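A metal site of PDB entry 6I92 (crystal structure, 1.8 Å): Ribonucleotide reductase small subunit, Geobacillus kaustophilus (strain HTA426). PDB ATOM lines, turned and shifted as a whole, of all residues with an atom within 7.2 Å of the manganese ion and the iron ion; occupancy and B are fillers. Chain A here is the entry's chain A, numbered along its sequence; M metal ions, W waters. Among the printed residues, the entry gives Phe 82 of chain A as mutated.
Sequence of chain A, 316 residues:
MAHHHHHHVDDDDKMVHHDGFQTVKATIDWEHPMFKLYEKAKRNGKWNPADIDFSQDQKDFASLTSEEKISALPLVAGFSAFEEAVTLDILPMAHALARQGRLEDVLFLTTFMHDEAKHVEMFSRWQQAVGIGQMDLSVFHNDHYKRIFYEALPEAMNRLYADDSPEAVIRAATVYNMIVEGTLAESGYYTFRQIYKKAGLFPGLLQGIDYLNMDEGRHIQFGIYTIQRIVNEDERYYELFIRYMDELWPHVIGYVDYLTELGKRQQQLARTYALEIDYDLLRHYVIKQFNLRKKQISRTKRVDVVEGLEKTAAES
Five residues have an atom within 4 Å of the manganese ion: Glu 83, Glu 116, His 119, Glu 181 and Glu 216.
The side-chain carboxylate of Asp 115 is in hydrogen-bond range of a ring nitrogen (NE2) of His 219 (3.1 Å).
O of Glu 116 is in hydrogen-bond range of OG1 of Thr 87 (3.2 Å).
The backbone carbonyl oxygen (O) of Glu 83 is in hydrogen-bond range of the side-chain hydroxyl (OG1) of Thr 87, at 2.7 Å.
OH of Tyr 189 is in hydrogen-bond range of OE2 of Glu 83, at 2.6 Å.
A ring nitrogen (NE2) of His 119 sits close to the backbone carbonyl oxygen (O) of Asp 115 (3.3 Å).
A ring nitrogen (NE2) of His 119 lies within hydrogen-bond range of the side-chain carboxylate of Asp 215 (2.7 Å).
The backbone NH of Glu 181 sits at hydrogen-bond distance from the backbone carbonyl oxygen of Tyr 176 (3.0 Å).
The iron ion is bound by OE2 of Glu 181 (1.9 Å), ND1 of His 219 (2.0 Å), OE2 of Glu 116 (2.1 Å), OE1 of Glu 181 (2.1 Å), OE1 of Glu 216 (2.1 Å) and OE2 of Glu 216 (2.3 Å).
The iron ion has six donor atoms within binding distance.
The manganese ion is bound by water W1 (1.9 Å).
OE1 of Glu 83 binds the manganese ion (2.1 Å).
The side-chain carboxylate (OE1) of Glu 116 binds the manganese ion.
The manganese ion is bound by OE2 of Glu 216 (2.2 Å).
The manganese ion is bound by ND1 of His 119.
The manganese ion has five donor atoms within binding distance.
Merely in contact with the iron ion: Phe 112 (3.9 Å).
The nearest printed residue that does not touch the iron ion is Tyr 176 (4.9 Å).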
ATOM      1  N   PHE A  82     -35.688  17.444  21.511  1.00  0.00           N
ATOM      2  CA  PHE A  82     -34.829  17.058  22.620  1.00  0.00           C
ATOM      3  C   PHE A  82     -33.878  18.220  22.903  1.00  0.00           C
ATOM      4  O   PHE A  82     -33.784  18.713  24.026  1.00  0.00           O
ATOM      5  CB  PHE A  82     -33.985  15.796  22.336  1.00  0.00           C
ATOM      6  CG  PHE A  82     -34.751  14.474  22.286  1.00  0.00           C
ATOM      7  CD1 PHE A  82     -36.057  14.349  22.736  1.00  0.00           C
ATOM      8  CD2 PHE A  82     -34.112  13.338  21.790  1.00  0.00           C
ATOM      9  CE1 PHE A  82     -36.714  13.104  22.680  1.00  0.00           C
ATOM     10  CE2 PHE A  82     -34.776  12.082  21.729  1.00  0.00           C
ATOM     11  CZ  PHE A  82     -36.058  11.972  22.171  1.00  0.00           C
ATOM     12  N   GLU A  83     -33.178  18.691  21.864  1.00  0.00           N
ATOM     13  CA  GLU A  83     -32.043  19.582  22.075  1.00  0.00           C
ATOM     14  C   GLU A  83     -32.466  21.010  22.395  1.00  0.00           C
ATOM     15  O   GLU A  83     -31.820  21.705  23.209  1.00  0.00           O
ATOM     16  CB  GLU A  83     -31.138  19.546  20.850  1.00  0.00           C
ATOM     17  CG  GLU A  83     -30.608  18.151  20.559  1.00  0.00           C
ATOM     18  CD  GLU A  83     -29.801  17.543  21.708  1.00  0.00           C
ATOM     19  OE1 GLU A  83     -29.162  18.301  22.520  1.00  0.00           O
ATOM     20  OE2 GLU A  83     -29.805  16.303  21.809  1.00  0.00           O
ATOM     21  N   VAL A  86     -33.649  21.118  26.158  1.00  0.00           N
ATOM     22  CA  VAL A  86     -32.606  21.061  27.187  1.00  0.00           C
ATOM     23  C   VAL A  86     -31.725  22.313  27.145  1.00  0.00           C
ATOM     24  O   VAL A  86     -31.199  22.746  28.184  1.00  0.00           O
ATOM     25  CB  VAL A  86     -31.779  19.747  27.075  1.00  0.00           C
ATOM     26  CG1 VAL A  86     -32.680  18.520  27.307  1.00  0.00           C
ATOM     27  CG2 VAL A  86     -31.042  19.621  25.762  1.00  0.00           C
ATOM     28  N   THR A  87     -31.599  22.964  25.994  1.00  0.00           N
ATOM     29  CA  THR A  87     -30.883  24.233  25.963  1.00  0.00           C
ATOM     30  C   THR A  87     -31.561  25.249  26.858  1.00  0.00           C
ATOM     31  O   THR A  87     -30.909  25.932  27.669  1.00  0.00           O
ATOM     32  CB  THR A  87     -30.809  24.793  24.521  1.00  0.00           C
ATOM     33  OG1 THR A  87     -30.167  23.844  23.671  1.00  0.00           O
ATOM     34  CG2 THR A  87     -29.990  26.102  24.456  1.00  0.00           C
ATOM     35  N   PHE A 112     -21.959  23.111  29.635  1.00  0.00           N
ATOM     36  CA  PHE A 112     -23.173  22.317  29.396  1.00  0.00           C
ATOM     37  C   PHE A 112     -24.140  23.066  28.492  1.00  0.00           C
ATOM     38  O   PHE A 112     -24.616  22.528  27.477  1.00  0.00           O
ATOM     39  CB  PHE A 112     -23.793  22.006  30.773  1.00  0.00           C
ATOM     40  CG  PHE A 112     -24.851  20.924  30.817  1.00  0.00           C
ATOM     41  CD1 PHE A 112     -24.743  19.922  31.754  1.00  0.00           C
ATOM     42  CD2 PHE A 112     -26.010  20.979  30.067  1.00  0.00           C
ATOM     43  CE1 PHE A 112     -25.741  18.948  31.903  1.00  0.00           C
ATOM     44  CE2 PHE A 112     -27.005  20.025  30.211  1.00  0.00           C
ATOM     45  CZ  PHE A 112     -26.862  18.994  31.138  1.00  0.00           C
ATOM     46  N   ASP A 115     -22.868  23.528  24.922  1.00  0.00           N
ATOM     47  CA  ASP A 115     -22.993  22.250  24.194  1.00  0.00           C
ATOM     48  C   ASP A 115     -24.403  22.055  23.643  1.00  0.00           C
ATOM     49  O   ASP A 115     -24.587  21.669  22.474  1.00  0.00           O
ATOM     50  CB  ASP A 115     -22.627  21.048  25.097  1.00  0.00           C
ATOM     51  CG  ASP A 115     -21.171  20.947  25.470  1.00  0.00           C
ATOM     52  OD1 ASP A 115     -20.279  21.626  24.918  1.00  0.00           O
ATOM     53  OD2 ASP A 115     -20.890  20.111  26.381  1.00  0.00           O
ATOM     54  N   GLU A 116     -25.412  22.294  24.467  1.00  0.00           N
ATOM     55  CA  GLU A 116     -26.791  22.128  24.015  1.00  0.00           C
ATOM     56  C   GLU A 116     -27.100  23.100  22.869  1.00  0.00           C
ATOM     57  O   GLU A 116     -27.791  22.734  21.924  1.00  0.00           O
ATOM     58  CB  GLU A 116     -27.812  22.342  25.130  1.00  0.00           C
ATOM     59  CG  GLU A 116     -27.658  21.428  26.389  1.00  0.00           C
ATOM     60  CD  GLU A 116     -27.660  19.923  26.152  1.00  0.00           C
ATOM     61  OE1 GLU A 116     -27.760  19.455  24.992  1.00  0.00           O
ATOM     62  OE2 GLU A 116     -27.631  19.216  27.152  1.00  0.00           O
ATOM     63  N   ALA A 117     -26.598  24.340  22.942  1.00  0.00           N
ATOM     64  CA  ALA A 117     -26.762  25.263  21.805  1.00  0.00           C
ATOM     65  C   ALA A 117     -26.198  24.678  20.503  1.00  0.00           C
ATOM     66  O   ALA A 117     -26.821  24.771  19.438  1.00  0.00           O
ATOM     67  CB  ALA A 117     -26.096  26.615  22.107  1.00  0.00           C
ATOM     68  N   LYS A 118     -25.010  24.087  20.559  1.00  0.00           N
ATOM     69  CA  LYS A 118     -24.456  23.446  19.372  1.00  0.00           C
ATOM     70  C   LYS A 118     -25.311  22.275  18.928  1.00  0.00           C
ATOM     71  O   LYS A 118     -25.425  22.026  17.727  1.00  0.00           O
ATOM     72  CB  LYS A 118     -23.005  23.001  19.640  1.00  0.00           C
ATOM     73  CG  LYS A 118     -22.093  24.197  19.821  1.00  0.00           C
ATOM     74  CD  LYS A 118     -20.575  23.833  19.761  1.00  0.00           C
ATOM     75  CE  LYS A 118     -20.161  22.822  20.806  1.00  0.00           C
ATOM     76  NZ  LYS A 118     -18.695  22.676  20.898  1.00  0.00           N
ATOM     77  N   HIS A 119     -25.931  21.531  19.862  1.00  0.00           N
ATOM     78  CA  HIS A 119     -26.734  20.385  19.425  1.00  0.00           C
ATOM     79  C   HIS A 119     -28.004  20.858  18.712  1.00  0.00           C
ATOM     80  O   HIS A 119     -28.376  20.272  17.686  1.00  0.00           O
ATOM     81  CB  HIS A 119     -27.084  19.469  20.590  1.00  0.00           C
ATOM     82  CG  HIS A 119     -25.892  18.985  21.341  1.00  0.00           C
ATOM     83  ND1 HIS A 119     -25.982  18.427  22.605  1.00  0.00           N
ATOM     84  CD2 HIS A 119     -24.569  18.995  21.031  1.00  0.00           C
ATOM     85  CE1 HIS A 119     -24.769  18.146  23.036  1.00  0.00           C
ATOM     86  NE2 HIS A 119     -23.898  18.471  22.098  1.00  0.00           N
ATOM     87  N   VAL A 120     -28.630  21.920  19.206  1.00  0.00           N
ATOM     88  CA  VAL A 120     -29.775  22.526  18.519  1.00  0.00           C
ATOM     89  C   VAL A 120     -29.364  22.972  17.148  1.00  0.00           C
ATOM     90  O   VAL A 120     -30.081  22.763  16.153  1.00  0.00           O
ATOM     91  CB  VAL A 120     -30.328  23.748  19.306  1.00  0.00           C
ATOM     92  CG1 VAL A 120     -31.462  24.442  18.511  1.00  0.00           C
ATOM     93  CG2 VAL A 120     -30.872  23.367  20.607  1.00  0.00           C
ATOM     94  N   PHE A 123     -28.686  19.961  14.463  1.00  0.00           N
ATOM     95  CA  PHE A 123     -29.897  19.369  13.882  1.00  0.00           C
ATOM     96  C   PHE A 123     -30.636  20.351  12.964  1.00  0.00           C
ATOM     97  O   PHE A 123     -31.163  19.959  11.921  1.00  0.00           O
ATOM     98  CB  PHE A 123     -30.825  18.847  14.963  1.00  0.00           C
ATOM     99  CG  PHE A 123     -30.360  17.528  15.599  1.00  0.00           C
ATOM    100  CD1 PHE A 123     -30.164  16.398  14.810  1.00  0.00           C
ATOM    101  CD2 PHE A 123     -30.151  17.430  16.971  1.00  0.00           C
ATOM    102  CE1 PHE A 123     -29.734  15.207  15.394  1.00  0.00           C
ATOM    103  CE2 PHE A 123     -29.735  16.253  17.565  1.00  0.00           C
ATOM    104  CZ  PHE A 123     -29.515  15.139  16.768  1.00  0.00           C
ATOM    105  N   TYR A 176     -34.167  15.533  34.057  1.00  0.00           N
ATOM    106  CA  TYR A 176     -33.383  16.117  32.978  1.00  0.00           C
ATOM    107  C   TYR A 176     -32.223  15.195  32.563  1.00  0.00           C
ATOM    108  O   TYR A 176     -32.095  14.826  31.393  1.00  0.00           O
ATOM    109  CB  TYR A 176     -32.836  17.460  33.436  1.00  0.00           C
ATOM    110  CG  TYR A 176     -32.104  18.274  32.382  1.00  0.00           C
ATOM    111  CD1 TYR A 176     -32.622  19.485  31.964  1.00  0.00           C
ATOM    112  CD2 TYR A 176     -30.909  17.861  31.815  1.00  0.00           C
ATOM    113  CE1 TYR A 176     -31.965  20.245  30.987  1.00  0.00           C
ATOM    114  CE2 TYR A 176     -30.269  18.603  30.841  1.00  0.00           C
ATOM    115  CZ  TYR A 176     -30.805  19.799  30.439  1.00  0.00           C
ATOM    116  OH  TYR A 176     -30.150  20.562  29.476  1.00  0.00           O
ATOM    117  N   ASN A 177     -31.336  14.903  33.512  1.00  0.00           N
ATOM    118  CA  ASN A 177     -30.066  14.215  33.199  1.00  0.00           C
ATOM    119  C   ASN A 177     -30.260  12.705  33.086  1.00  0.00           C
ATOM    120  O   ASN A 177     -29.768  12.073  32.123  1.00  0.00           O
ATOM    121  CB  ASN A 177     -29.011  14.527  34.264  1.00  0.00           C
ATOM    122  CG  ASN A 177     -28.776  16.034  34.435  1.00  0.00           C
ATOM    123  OD1 ASN A 177     -29.273  16.652  35.378  1.00  0.00           O
ATOM    124  ND2 ASN A 177     -28.008  16.612  33.547  1.00  0.00           N
ATOM    125  N   GLU A 181     -31.927  12.929  29.094  1.00  0.00           N
ATOM    126  CA  GLU A 181     -30.667  12.783  28.382  1.00  0.00           C
ATOM    127  C   GLU A 181     -30.141  11.360  28.464  1.00  0.00           C
ATOM    128  O   GLU A 181     -29.759  10.774  27.454  1.00  0.00           O
ATOM    129  CB  GLU A 181     -29.618  13.775  28.888  1.00  0.00           C
ATOM    130  CG  GLU A 181     -30.011  15.280  28.656  1.00  0.00           C
ATOM    131  CD  GLU A 181     -28.867  16.222  28.233  1.00  0.00           C
ATOM    132  OE1 GLU A 181     -28.062  16.584  29.091  1.00  0.00           O
ATOM    133  OE2 GLU A 181     -28.805  16.625  27.047  1.00  0.00           O
ATOM    134  N   ALA A 185     -32.757  10.218  25.151  1.00  0.00           N
ATOM    135  CA  ALA A 185     -32.006  10.778  24.037  1.00  0.00           C
ATOM    136  C   ALA A 185     -30.850   9.850  23.689  1.00  0.00           C
ATOM    137  O   ALA A 185     -30.538   9.639  22.511  1.00  0.00           O
ATOM    138  CB  ALA A 185     -31.505  12.181  24.371  1.00  0.00           C
ATOM    139  N   TYR A 189     -30.275   8.248  19.901  1.00  0.00           N
ATOM    140  CA  TYR A 189     -29.128   8.522  19.049  1.00  0.00           C
ATOM    141  C   TYR A 189     -28.381   7.234  18.729  1.00  0.00           C
ATOM    142  O   TYR A 189     -27.903   7.055  17.609  1.00  0.00           O
ATOM    143  CB  TYR A 189     -28.189   9.537  19.726  1.00  0.00           C
ATOM    144  CG  TYR A 189     -28.843  10.906  19.824  1.00  0.00           C
ATOM    145  CD1 TYR A 189     -29.572  11.417  18.753  1.00  0.00           C
ATOM    146  CD2 TYR A 189     -28.811  11.638  21.005  1.00  0.00           C
ATOM    147  CE1 TYR A 189     -30.199  12.651  18.822  1.00  0.00           C
ATOM    148  CE2 TYR A 189     -29.456  12.880  21.100  1.00  0.00           C
ATOM    149  CZ  TYR A 189     -30.146  13.379  19.999  1.00  0.00           C
ATOM    150  OH  TYR A 189     -30.807  14.602  20.045  1.00  0.00           O
ATOM    151  N   LEU A 212     -21.945  15.059  19.493  1.00  0.00           N
ATOM    152  CA  LEU A 212     -22.979  15.236  20.484  1.00  0.00           C
ATOM    153  C   LEU A 212     -22.889  14.183  21.593  1.00  0.00           C
ATOM    154  O   LEU A 212     -23.011  14.492  22.778  1.00  0.00           O
ATOM    155  CB  LEU A 212     -24.330  15.174  19.782  1.00  0.00           C
ATOM    156  CG  LEU A 212     -25.581  15.327  20.575  1.00  0.00           C
ATOM    157  CD1 LEU A 212     -26.687  15.870  19.637  1.00  0.00           C
ATOM    158  CD2 LEU A 212     -26.014  13.975  21.235  1.00  0.00           C
ATOM    159  N   ASP A 215     -20.158  14.958  24.050  1.00  0.00           N
ATOM    160  CA  ASP A 215     -20.587  15.998  24.978  1.00  0.00           C
ATOM    161  C   ASP A 215     -21.485  15.432  26.067  1.00  0.00           C
ATOM    162  O   ASP A 215     -21.337  15.777  27.256  1.00  0.00           O
ATOM    163  CB  ASP A 215     -21.355  17.135  24.268  1.00  0.00           C
ATOM    164  CG  ASP A 215     -20.538  17.877  23.220  1.00  0.00           C
ATOM    165  OD1 ASP A 215     -19.315  18.003  23.354  1.00  0.00           O
ATOM    166  OD2 ASP A 215     -21.178  18.392  22.269  1.00  0.00           O
ATOM    167  N   GLU A 216     -22.468  14.623  25.678  1.00  0.00           N
ATOM    168  CA  GLU A 216     -23.467  14.159  26.604  1.00  0.00           C
ATOM    169  C   GLU A 216     -22.888  13.219  27.652  1.00  0.00           C
ATOM    170  O   GLU A 216     -23.440  13.121  28.736  1.00  0.00           O
ATOM    171  CB  GLU A 216     -24.639  13.518  25.834  1.00  0.00           C
ATOM    172  CG  GLU A 216     -25.459  14.543  24.961  1.00  0.00           C
ATOM    173  CD  GLU A 216     -26.041  15.635  25.798  1.00  0.00           C
ATOM    174  OE1 GLU A 216     -26.336  15.302  26.965  1.00  0.00           O
ATOM    175  OE2 GLU A 216     -26.255  16.767  25.270  1.00  0.00           O
ATOM    176  N   GLY A 217     -21.741  12.579  27.378  1.00  0.00           N
ATOM    177  CA  GLY A 217     -20.999  11.897  28.435  1.00  0.00           C
ATOM    178  C   GLY A 217     -20.709  12.785  29.640  1.00  0.00           C
ATOM    179  O   GLY A 217     -20.887  12.379  30.789  1.00  0.00           O
ATOM    180  N   ARG A 218     -20.239  14.009  29.398  1.00  0.00           N
ATOM    181  CA  ARG A 218     -20.031  14.938  30.509  1.00  0.00           C
ATOM    182  C   ARG A 218     -21.329  15.348  31.180  1.00  0.00           C
ATOM    183  O   ARG A 218     -21.362  15.529  32.401  1.00  0.00           O
ATOM    184  CB  ARG A 218     -19.283  16.191  30.024  1.00  0.00           C
ATOM    185  CG  ARG A 218     -17.950  15.863  29.417  1.00  0.00           C
ATOM    186  CD  ARG A 218     -17.141  17.139  29.162  1.00  0.00           C
ATOM    187  NE  ARG A 218     -17.839  17.984  28.166  1.00  0.00           N
ATOM    188  CZ  ARG A 218     -17.721  17.852  26.848  1.00  0.00           C
ATOM    189  NH1 ARG A 218     -16.900  16.949  26.311  1.00  0.00           N
ATOM    190  NH2 ARG A 218     -18.402  18.666  26.045  1.00  0.00           N
ATOM    191  N   HIS A 219     -22.394  15.570  30.401  1.00  0.00           N
ATOM    192  CA  HIS A 219     -23.630  16.037  30.993  1.00  0.00           C
ATOM    193  C   HIS A 219     -24.166  15.027  31.996  1.00  0.00           C
ATOM    194  O   HIS A 219     -24.658  15.391  33.054  1.00  0.00           O
ATOM    195  CB  HIS A 219     -24.696  16.272  29.909  1.00  0.00           C
ATOM    196  CG  HIS A 219     -24.315  17.327  28.919  1.00  0.00           C
ATOM    197  ND1 HIS A 219     -25.173  17.761  27.931  1.00  0.00           N
ATOM    198  CD2 HIS A 219     -23.184  18.040  28.800  1.00  0.00           C
ATOM    199  CE1 HIS A 219     -24.546  18.665  27.201  1.00  0.00           C
ATOM    200  NE2 HIS A 219     -23.346  18.872  27.722  1.00  0.00           N
ATOM    201  N   ILE A 220     -24.065  13.746  31.665  1.00  0.00           N
ATOM    202  CA  ILE A 220     -24.608  12.736  32.571  1.00  0.00           C
ATOM    203  C   ILE A 220     -23.782  12.682  33.843  1.00  0.00           C
ATOM    204  O   ILE A 220     -24.317  12.418  34.934  1.00  0.00           O
ATOM    205  CB  ILE A 220     -24.681  11.363  31.867  1.00  0.00           C
ATOM    206  CG1 ILE A 220     -25.372  10.336  32.788  1.00  0.00           C
ATOM    207  CG2 ILE A 220     -23.275  10.849  31.492  1.00  0.00           C
ATOM    208  CD1 ILE A 220     -26.874  10.659  32.992  1.00  0.00           C
HETATM  209 MN    MN M   1     -27.656  17.685  23.843  1.00  0.00          MN
HETATM  210 FE    FE M   2     -27.016  17.261  27.407  1.00  0.00          FE
HETATM  211  O   HOH W   1     -28.269  15.879  23.491  1.00  0.00           O
